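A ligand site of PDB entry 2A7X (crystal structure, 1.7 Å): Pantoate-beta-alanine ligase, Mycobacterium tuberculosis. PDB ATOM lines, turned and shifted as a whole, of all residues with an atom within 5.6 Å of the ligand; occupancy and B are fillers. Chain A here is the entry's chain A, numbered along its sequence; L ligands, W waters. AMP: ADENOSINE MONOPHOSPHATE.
Merely in contact with the ligand: Pro 38, Thr 39, His 44, Gly 46, Leu 50, Phe 157, Lys 160, Gln 164, Pro 185 and Thr 186. Hydrophobic or aromatic side chains within 4 Å of the ligand: Met 40, His 44, His 47, Leu 50, Phe 157, Val 187 and Met 195. Within 4 Å of the ligand: Pro 38, Thr 39, Met 40, His 44, Gly 46, His 47, Leu 50, Phe 157, Gly 158, Lys 160, Asp 161, Gln 164, Pro 185, Thr 186, Val 187 and Met 195. The nearest printed residue that does not touch the ligand is Gly 41 (4.1 Å).
An oxygen (O2') of the ligand lies within hydrogen-bond range of the side-chain carboxylate of Asp 161 (2.6 Å). The backbone carbonyl oxygen of Met 195 sits at hydrogen-bond distance from a nitrogen (N6) of the ligand (2.9 Å). N of Gly 158 is in hydrogen-bond range of O3' of the ligand, at 2.9 Å. O of Gly 158 lies within hydrogen-bond range of O2' of the ligand (3.4 Å). The backbone NH of Val 187 sits at hydrogen-bond distance from a nitrogen (N1) of the ligand (2.9 Å). A nitrogen (N6) of the ligand sits at hydrogen-bond distance from the backbone carbonyl oxygen (O) of Val 187, 3.0 Å away. O2P of the ligand lies within hydrogen-bond range of NE2 of His 47. The backbone NH (N) of Met 40 lies within hydrogen-bond range of an oxygen (O2P) of the ligand.
The backbone NH of Met 195 is in hydrogen-bond range of the backbone carbonyl oxygen of Val 187. The backbone NH (N) of His 44 lies within hydrogen-bond range of a ring nitrogen (ND1) of His 47, at 3.0 Å. ND1 of His 44 is in hydrogen-bond range of N of Gly 46. N of Val 184 is in hydrogen-bond range of O of Phe 157 (2.9 Å). The side-chain hydroxyl of Thr 186 sits at hydrogen-bond distance from the backbone NH of Lys 160. The side-chain hydroxyl (OG1) of Thr 39 lies within hydrogen-bond range of the backbone NH (N) of Gly 41, 3.1 Å away.
Water W2 bridges an oxygen (O1P) of the ligand (2.5 Å) and the side-chain hydroxyl of Ser 197 (2.9 Å). Water W5 lies within hydrogen-bond range of O3' of the ligand, O of Pro 38 and O of Phe 156. Water W4 lies within hydrogen-bond range of the side-chain carboxylate of Asp 161 and an oxygen (O1P) of the ligand. Water W1 lies within hydrogen-bond range of N7 of the ligand, O of Met 195 and OG of Ser 196. Water W3 lies within hydrogen-bond range of O of Gly 41 (2.7 Å), O2P of the ligand (3.0 Å), OG of Ser 197 (3.3 Å) and NE2 of His 47 (3.5 Å). Water W6 lies within hydrogen-bond range of O of Gly 158 (2.8 Å), NE2 of Gln 164 (3.0 Å), O of Asp 161 (3.0 Å) and O2' of the ligand (3.4 Å).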
ATOM      1  N   PRO A  38     -30.618  15.011 -22.486  1.00  0.00           N
ATOM      2  CA  PRO A  38     -29.914  16.087 -21.787  1.00  0.00           C
ATOM      3  C   PRO A  38     -28.542  15.700 -21.320  1.00  0.00           C
ATOM      4  O   PRO A  38     -28.357  14.632 -20.724  1.00  0.00           O
ATOM      5  CB  PRO A  38     -30.800  16.409 -20.574  1.00  0.00           C
ATOM      6  CG  PRO A  38     -32.173  15.923 -20.981  1.00  0.00           C
ATOM      7  CD  PRO A  38     -31.843  14.571 -21.751  1.00  0.00           C
ATOM      8  N   THR A  39     -27.563  16.559 -21.603  1.00  0.00           N
ATOM      9  CA  THR A  39     -26.186  16.302 -21.120  1.00  0.00           C
ATOM     10  C   THR A  39     -25.496  17.582 -20.715  1.00  0.00           C
ATOM     11  O   THR A  39     -25.981  18.685 -20.996  1.00  0.00           O
ATOM     12  CB  THR A  39     -25.274  15.677 -22.224  1.00  0.00           C
ATOM     13  OG1 THR A  39     -24.866  16.752 -23.133  1.00  0.00           O
ATOM     14  CG2 THR A  39     -26.012  14.601 -23.032  1.00  0.00           C
ATOM     15  N   MET A  40     -24.364  17.385 -20.064  1.00  0.00           N
ATOM     16  CA  MET A  40     -23.471  18.519 -19.745  1.00  0.00           C
ATOM     17  C   MET A  40     -22.236  18.535 -20.628  1.00  0.00           C
ATOM     18  O   MET A  40     -21.199  19.144 -20.278  1.00  0.00           O
ATOM     19  CB  MET A  40     -23.097  18.501 -18.248  1.00  0.00           C
ATOM     20  CG  MET A  40     -24.321  18.782 -17.386  1.00  0.00           C
ATOM     21  SD  MET A  40     -23.824  19.067 -15.623  1.00  0.00           S
ATOM     22  CE  MET A  40     -22.827  17.630 -15.354  1.00  0.00           C
ATOM     23  N   GLY A  41     -22.338  17.913 -21.789  1.00  0.00           N
ATOM     24  CA  GLY A  41     -21.191  17.797 -22.714  1.00  0.00           C
ATOM     25  C   GLY A  41     -20.083  16.906 -22.143  1.00  0.00           C
ATOM     26  O   GLY A  41     -20.312  16.089 -21.239  1.00  0.00           O
ATOM     27  N   HIS A  44     -19.001  10.909 -23.619  1.00  0.00           N
ATOM     28  CA  HIS A  44     -18.317   9.613 -23.718  1.00  0.00           C
ATOM     29  C   HIS A  44     -19.334   8.516 -24.014  1.00  0.00           C
ATOM     30  O   HIS A  44     -20.531   8.816 -24.243  1.00  0.00           O
ATOM     31  CB  HIS A  44     -17.586   9.307 -22.387  1.00  0.00           C
ATOM     32  CG  HIS A  44     -18.471   9.424 -21.194  1.00  0.00           C
ATOM     33  ND1 HIS A  44     -19.460   8.512 -20.916  1.00  0.00           N
ATOM     34  CD2 HIS A  44     -18.544  10.357 -20.223  1.00  0.00           C
ATOM     35  CE1 HIS A  44     -20.086   8.858 -19.802  1.00  0.00           C
ATOM     36  NE2 HIS A  44     -19.562   9.990 -19.373  1.00  0.00           N
ATOM     37  N   GLY A  46     -20.908   6.455 -22.325  1.00  0.00           N
ATOM     38  CA  GLY A  46     -22.112   6.418 -21.469  1.00  0.00           C
ATOM     39  C   GLY A  46     -23.187   7.317 -22.075  1.00  0.00           C
ATOM     40  O   GLY A  46     -24.336   6.908 -22.244  1.00  0.00           O
ATOM     41  N   HIS A  47     -22.807   8.523 -22.495  1.00  0.00           N
ATOM     42  CA  HIS A  47     -23.769   9.385 -23.197  1.00  0.00           C
ATOM     43  C   HIS A  47     -24.217   8.778 -24.492  1.00  0.00           C
ATOM     44  O   HIS A  47     -25.393   8.906 -24.867  1.00  0.00           O
ATOM     45  CB  HIS A  47     -23.151  10.733 -23.543  1.00  0.00           C
ATOM     46  CG  HIS A  47     -22.715  11.519 -22.349  1.00  0.00           C
ATOM     47  ND1 HIS A  47     -21.394  11.649 -22.021  1.00  0.00           N
ATOM     48  CD2 HIS A  47     -23.413  12.167 -21.394  1.00  0.00           C
ATOM     49  CE1 HIS A  47     -21.281  12.369 -20.913  1.00  0.00           C
ATOM     50  NE2 HIS A  47     -22.491  12.723 -20.527  1.00  0.00           N
ATOM     51  N   ALA A  49     -24.687   5.790 -25.318  1.00  0.00           N
ATOM     52  CA  ALA A  49     -25.715   4.767 -25.104  1.00  0.00           C
ATOM     53  C   ALA A  49     -27.110   5.416 -25.064  1.00  0.00           C
ATOM     54  O   ALA A  49     -28.073   4.829 -25.633  1.00  0.00           O
ATOM     55  CB  ALA A  49     -25.457   3.956 -23.825  1.00  0.00           C
ATOM     56  N   LEU A  50     -27.217   6.582 -24.399  1.00  0.00           N
ATOM     57  CA  LEU A  50     -28.511   7.310 -24.385  1.00  0.00           C
ATOM     58  C   LEU A  50     -28.870   7.701 -25.795  1.00  0.00           C
ATOM     59  O   LEU A  50     -29.984   7.517 -26.214  1.00  0.00           O
ATOM     60  CB  LEU A  50     -28.444   8.525 -23.488  1.00  0.00           C
ATOM     61  CG  LEU A  50     -28.653   8.237 -21.982  1.00  0.00           C
ATOM     62  CD1 LEU A  50     -27.705   7.257 -21.330  1.00  0.00           C
ATOM     63  CD2 LEU A  50     -28.627   9.599 -21.298  1.00  0.00           C
ATOM     64  N   PHE A 156     -34.358  10.778 -22.204  1.00  0.00           N
ATOM     65  CA  PHE A 156     -33.504   9.633 -21.802  1.00  0.00           C
ATOM     66  C   PHE A 156     -32.556  10.092 -20.731  1.00  0.00           C
ATOM     67  O   PHE A 156     -31.898  11.139 -20.853  1.00  0.00           O
ATOM     68  CB  PHE A 156     -32.681   9.171 -23.041  1.00  0.00           C
ATOM     69  CG  PHE A 156     -33.562   8.585 -24.100  1.00  0.00           C
ATOM     70  CD1 PHE A 156     -34.363   9.375 -24.927  1.00  0.00           C
ATOM     71  CD2 PHE A 156     -33.693   7.222 -24.197  1.00  0.00           C
ATOM     72  CE1 PHE A 156     -35.262   8.765 -25.863  1.00  0.00           C
ATOM     73  CE2 PHE A 156     -34.614   6.623 -25.139  1.00  0.00           C
ATOM     74  CZ  PHE A 156     -35.381   7.413 -25.923  1.00  0.00           C
ATOM     75  N   PHE A 157     -32.489   9.274 -19.657  1.00  0.00           N
ATOM     76  CA  PHE A 157     -31.564   9.553 -18.528  1.00  0.00           C
ATOM     77  C   PHE A 157     -30.834   8.247 -18.167  1.00  0.00           C
ATOM     78  O   PHE A 157     -31.430   7.186 -18.250  1.00  0.00           O
ATOM     79  CB  PHE A 157     -32.362  10.034 -17.325  1.00  0.00           C
ATOM     80  CG  PHE A 157     -32.857  11.470 -17.476  1.00  0.00           C
ATOM     81  CD1 PHE A 157     -34.129  11.738 -17.966  1.00  0.00           C
ATOM     82  CD2 PHE A 157     -32.009  12.515 -17.116  1.00  0.00           C
ATOM     83  CE1 PHE A 157     -34.531  13.095 -18.117  1.00  0.00           C
ATOM     84  CE2 PHE A 157     -32.389  13.862 -17.261  1.00  0.00           C
ATOM     85  CZ  PHE A 157     -33.648  14.131 -17.778  1.00  0.00           C
ATOM     86  N   GLY A 158     -29.602   8.362 -17.705  1.00  0.00           N
ATOM     87  CA  GLY A 158     -28.874   7.163 -17.407  1.00  0.00           C
ATOM     88  C   GLY A 158     -29.164   6.695 -15.997  1.00  0.00           C
ATOM     89  O   GLY A 158     -29.373   7.494 -15.083  1.00  0.00           O
ATOM     90  N   GLU A 159     -29.106   5.364 -15.808  1.00  0.00           N
ATOM     91  CA  GLU A 159     -29.209   4.800 -14.460  1.00  0.00           C
ATOM     92  C   GLU A 159     -27.978   5.185 -13.633  1.00  0.00           C
ATOM     93  O   GLU A 159     -28.002   5.096 -12.392  1.00  0.00           O
ATOM     94  CB  GLU A 159     -29.353   3.266 -14.504  1.00  0.00           C
ATOM     95  CG  GLU A 159     -30.739   2.860 -14.995  1.00  0.00           C
ATOM     96  CD  GLU A 159     -30.961   1.355 -14.965  1.00  0.00           C
ATOM     97  OE1 GLU A 159     -30.097   0.586 -14.496  1.00  0.00           O
ATOM     98  OE2 GLU A 159     -32.056   0.943 -15.404  1.00  0.00           O
ATOM     99  N   LYS A 160     -26.932   5.619 -14.326  1.00  0.00           N
ATOM    100  CA  LYS A 160     -25.697   6.078 -13.664  1.00  0.00           C
ATOM    101  C   LYS A 160     -26.093   7.081 -12.575  1.00  0.00           C
ATOM    102  O   LYS A 160     -25.591   7.019 -11.430  1.00  0.00           O
ATOM    103  CB  LYS A 160     -24.787   6.774 -14.700  1.00  0.00           C
ATOM    104  CG  LYS A 160     -23.562   7.476 -14.136  1.00  0.00           C
ATOM    105  CD  LYS A 160     -22.445   6.484 -13.925  1.00  0.00           C
ATOM    106  CE  LYS A 160     -21.193   7.136 -13.313  1.00  0.00           C
ATOM    107  NZ  LYS A 160     -21.468   7.741 -11.958  1.00  0.00           N
ATOM    108  N   ASP A 161     -26.961   8.036 -12.952  1.00  0.00           N
ATOM    109  CA  ASP A 161     -27.466   9.017 -11.962  1.00  0.00           C
ATOM    110  C   ASP A 161     -28.860   8.596 -11.512  1.00  0.00           C
ATOM    111  O   ASP A 161     -29.890   9.180 -11.903  1.00  0.00           O
ATOM    112  CB  ASP A 161     -27.420  10.401 -12.565  1.00  0.00           C
ATOM    113  CG  ASP A 161     -25.999  10.752 -12.961  1.00  0.00           C
ATOM    114  OD1 ASP A 161     -25.239  11.171 -12.064  1.00  0.00           O
ATOM    115  OD2 ASP A 161     -25.586  10.607 -14.121  1.00  0.00           O
ATOM    116  N   GLN A 164     -31.083  11.007  -9.654  1.00  0.00           N
ATOM    117  CA  GLN A 164     -31.592  11.999 -10.641  1.00  0.00           C
ATOM    118  C   GLN A 164     -32.750  11.439 -11.444  1.00  0.00           C
ATOM    119  O   GLN A 164     -33.800  12.088 -11.594  1.00  0.00           O
ATOM    120  CB  GLN A 164     -30.493  12.421 -11.601  1.00  0.00           C
ATOM    121  CG  GLN A 164     -30.961  13.283 -12.764  1.00  0.00           C
ATOM    122  CD  GLN A 164     -29.757  13.833 -13.523  1.00  0.00           C
ATOM    123  OE1 GLN A 164     -29.224  14.873 -13.115  1.00  0.00           O
ATOM    124  NE2 GLN A 164     -29.234  13.063 -14.502  1.00  0.00           N
ATOM    125  N   VAL A 184     -31.719   4.403 -19.012  1.00  0.00           N
ATOM    126  CA  VAL A 184     -30.819   3.607 -19.854  1.00  0.00           C
ATOM    127  C   VAL A 184     -29.747   3.003 -18.902  1.00  0.00           C
ATOM    128  O   VAL A 184     -29.201   3.713 -18.033  1.00  0.00           O
ATOM    129  CB  VAL A 184     -30.154   4.524 -20.876  1.00  0.00           C
ATOM    130  CG1 VAL A 184     -29.117   3.790 -21.686  1.00  0.00           C
ATOM    131  CG2 VAL A 184     -31.234   5.193 -21.822  1.00  0.00           C
ATOM    132  N   PRO A 185     -29.461   1.717 -19.026  1.00  0.00           N
ATOM    133  CA  PRO A 185     -28.473   1.074 -18.121  1.00  0.00           C
ATOM    134  C   PRO A 185     -27.096   1.724 -18.168  1.00  0.00           C
ATOM    135  O   PRO A 185     -26.684   2.325 -19.186  1.00  0.00           O
ATOM    136  CB  PRO A 185     -28.374  -0.333 -18.683  1.00  0.00           C
ATOM    137  CG  PRO A 185     -29.801  -0.538 -19.347  1.00  0.00           C
ATOM    138  CD  PRO A 185     -30.058   0.761 -19.994  1.00  0.00           C
ATOM    139  N   THR A 186     -26.402   1.597 -17.050  1.00  0.00           N
ATOM    140  CA  THR A 186     -25.089   2.215 -16.911  1.00  0.00           C
ATOM    141  C   THR A 186     -24.080   1.532 -17.836  1.00  0.00           C
ATOM    142  O   THR A 186     -23.959   0.296 -17.838  1.00  0.00           O
ATOM    143  CB  THR A 186     -24.646   2.090 -15.474  1.00  0.00           C
ATOM    144  OG1 THR A 186     -25.511   2.913 -14.673  1.00  0.00           O
ATOM    145  CG2 THR A 186     -23.193   2.629 -15.319  1.00  0.00           C
ATOM    146  N   VAL A 187     -23.320   2.344 -18.565  1.00  0.00           N
ATOM    147  CA  VAL A 187     -22.251   1.852 -19.400  1.00  0.00           C
ATOM    148  C   VAL A 187     -20.968   1.791 -18.576  1.00  0.00           C
ATOM    149  O   VAL A 187     -20.622   2.783 -17.891  1.00  0.00           O
ATOM    150  CB  VAL A 187     -22.011   2.766 -20.632  1.00  0.00           C
ATOM    151  CG1 VAL A 187     -20.851   2.256 -21.472  1.00  0.00           C
ATOM    152  CG2 VAL A 187     -23.250   2.888 -21.554  1.00  0.00           C
ATOM    153  N   ARG A 188     -20.295   0.647 -18.658  1.00  0.00           N
ATOM    154  CA  ARG A 188     -19.110   0.429 -17.789  1.00  0.00           C
ATOM    155  C   ARG A 188     -17.897   0.076 -18.648  1.00  0.00           C
ATOM    156  O   ARG A 188     -18.040  -0.488 -19.767  1.00  0.00           O
ATOM    157  CB  ARG A 188     -19.380  -0.744 -16.825  1.00  0.00           C
ATOM    158  CG  ARG A 188     -20.576  -0.495 -15.888  1.00  0.00           C
ATOM    159  CD  ARG A 188     -20.938  -1.687 -15.006  1.00  0.00           C
ATOM    160  NE  ARG A 188     -22.056  -1.332 -14.116  1.00  0.00           N
ATOM    161  CZ  ARG A 188     -21.919  -0.674 -12.966  1.00  0.00           C
ATOM    162  NH1 ARG A 188     -20.697  -0.297 -12.541  1.00  0.00           N
ATOM    163  NH2 ARG A 188     -23.003  -0.400 -12.196  1.00  0.00           N
ATOM    164  N   ALA A 194     -17.934   2.349 -13.751  1.00  0.00           N
ATOM    165  CA  ALA A 194     -18.984   3.097 -14.434  1.00  0.00           C
ATOM    166  C   ALA A 194     -18.363   4.275 -15.195  1.00  0.00           C
ATOM    167  O   ALA A 194     -17.616   5.088 -14.624  1.00  0.00           O
ATOM    168  CB  ALA A 194     -19.950   3.617 -13.347  1.00  0.00           C
ATOM    169  N   MET A 195     -18.644   4.394 -16.479  1.00  0.00           N
ATOM    170  CA  MET A 195     -18.065   5.531 -17.213  1.00  0.00           C
ATOM    171  C   MET A 195     -18.563   6.895 -16.717  1.00  0.00           C
ATOM    172  O   MET A 195     -19.739   7.086 -16.374  1.00  0.00           O
ATOM    173  CB  MET A 195     -18.320   5.392 -18.719  1.00  0.00           C
ATOM    174  CG  MET A 195     -17.515   4.198 -19.274  1.00  0.00           C
ATOM    175  SD  MET A 195     -17.739   4.235 -21.049  1.00  0.00           S
ATOM    176  CE  MET A 195     -16.918   2.667 -21.383  1.00  0.00           C
ATOM    177  N   SER A 196     -17.622   7.850 -16.661  1.00  0.00           N
ATOM    178  CA  SER A 196     -17.954   9.218 -16.214  1.00  0.00           C
ATOM    179  C   SER A 196     -16.836  10.131 -16.660  1.00  0.00           C
ATOM    180  O   SER A 196     -15.671   9.743 -16.658  1.00  0.00           O
ATOM    181  CB  SER A 196     -18.077   9.268 -14.680  1.00  0.00           C
ATOM    182  OG  SER A 196     -18.141  10.612 -14.245  1.00  0.00           O
ATOM    183  N   SER A 197     -17.210  11.357 -17.026  1.00  0.00           N
ATOM    184  CA  SER A 197     -16.177  12.348 -17.343  1.00  0.00           C
ATOM    185  C   SER A 197     -15.225  12.568 -16.162  1.00  0.00           C
ATOM    186  O   SER A 197     -14.050  12.924 -16.362  1.00  0.00           O
ATOM    187  CB  SER A 197     -16.818  13.669 -17.804  1.00  0.00           C
ATOM    188  OG  SER A 197     -17.839  14.136 -16.936  1.00  0.00           O
HETATM  189  P   AMP L   1     -24.048  14.382 -17.509  1.00  0.00           P
HETATM  190  O1P AMP L   1     -23.076  13.799 -16.549  1.00  0.00           O
HETATM  191  O2P AMP L   1     -23.464  14.884 -18.845  1.00  0.00           O
HETATM  192  O3P AMP L   1     -25.164  15.323 -17.069  1.00  0.00           O
HETATM  193  O5' AMP L   1     -24.849  13.041 -17.900  1.00  0.00           O
HETATM  194  C5' AMP L   1     -25.837  13.153 -18.931  1.00  0.00           C
HETATM  195  C4' AMP L   1     -26.725  11.926 -18.940  1.00  0.00           C
HETATM  196  O4' AMP L   1     -25.835  10.834 -19.312  1.00  0.00           O
HETATM  197  C3' AMP L   1     -27.288  11.620 -17.577  1.00  0.00           C
HETATM  198  O3' AMP L   1     -28.590  11.046 -17.843  1.00  0.00           O
HETATM  199  C2' AMP L   1     -26.366  10.520 -17.080  1.00  0.00           C
HETATM  200  O2' AMP L   1     -27.004   9.670 -16.109  1.00  0.00           O
HETATM  201  C1' AMP L   1     -26.023   9.798 -18.394  1.00  0.00           C
HETATM  202  N9  AMP L   1     -24.756   9.085 -18.194  1.00  0.00           N
HETATM  203  C8  AMP L   1     -23.543   9.580 -17.864  1.00  0.00           C
HETATM  204  N7  AMP L   1     -22.635   8.567 -17.737  1.00  0.00           N
HETATM  205  C5  AMP L   1     -23.330   7.418 -17.990  1.00  0.00           C
HETATM  206  C6  AMP L   1     -23.039   5.983 -18.019  1.00  0.00           C
HETATM  207  N6  AMP L   1     -21.772   5.577 -17.708  1.00  0.00           N
HETATM  208  N1  AMP L   1     -24.042   5.131 -18.367  1.00  0.00           N
HETATM  209  C2  AMP L   1     -25.334   5.518 -18.643  1.00  0.00           C
HETATM  210  N3  AMP L   1     -25.633   6.830 -18.609  1.00  0.00           N
HETATM  211  C4  AMP L   1     -24.713   7.770 -18.300  1.00  0.00           C
HETATM  212  O   HOH W   1     -21.136   9.767 -15.489  1.00  0.00           O
HETATM  213  O   HOH W   2     -20.619  14.318 -16.152  1.00  0.00           O
HETATM  214  O   HOH W   3     -20.498  14.975 -18.762  1.00  0.00           O
HETATM  215  O   HOH W   4     -23.183  11.370 -15.059  1.00  0.00           O
HETATM  216  O   HOH W   5     -29.869  12.646 -19.561  1.00  0.00           O
HETATM  217  O   HOH W   6     -30.099  10.207 -14.720  1.00  0.00           O
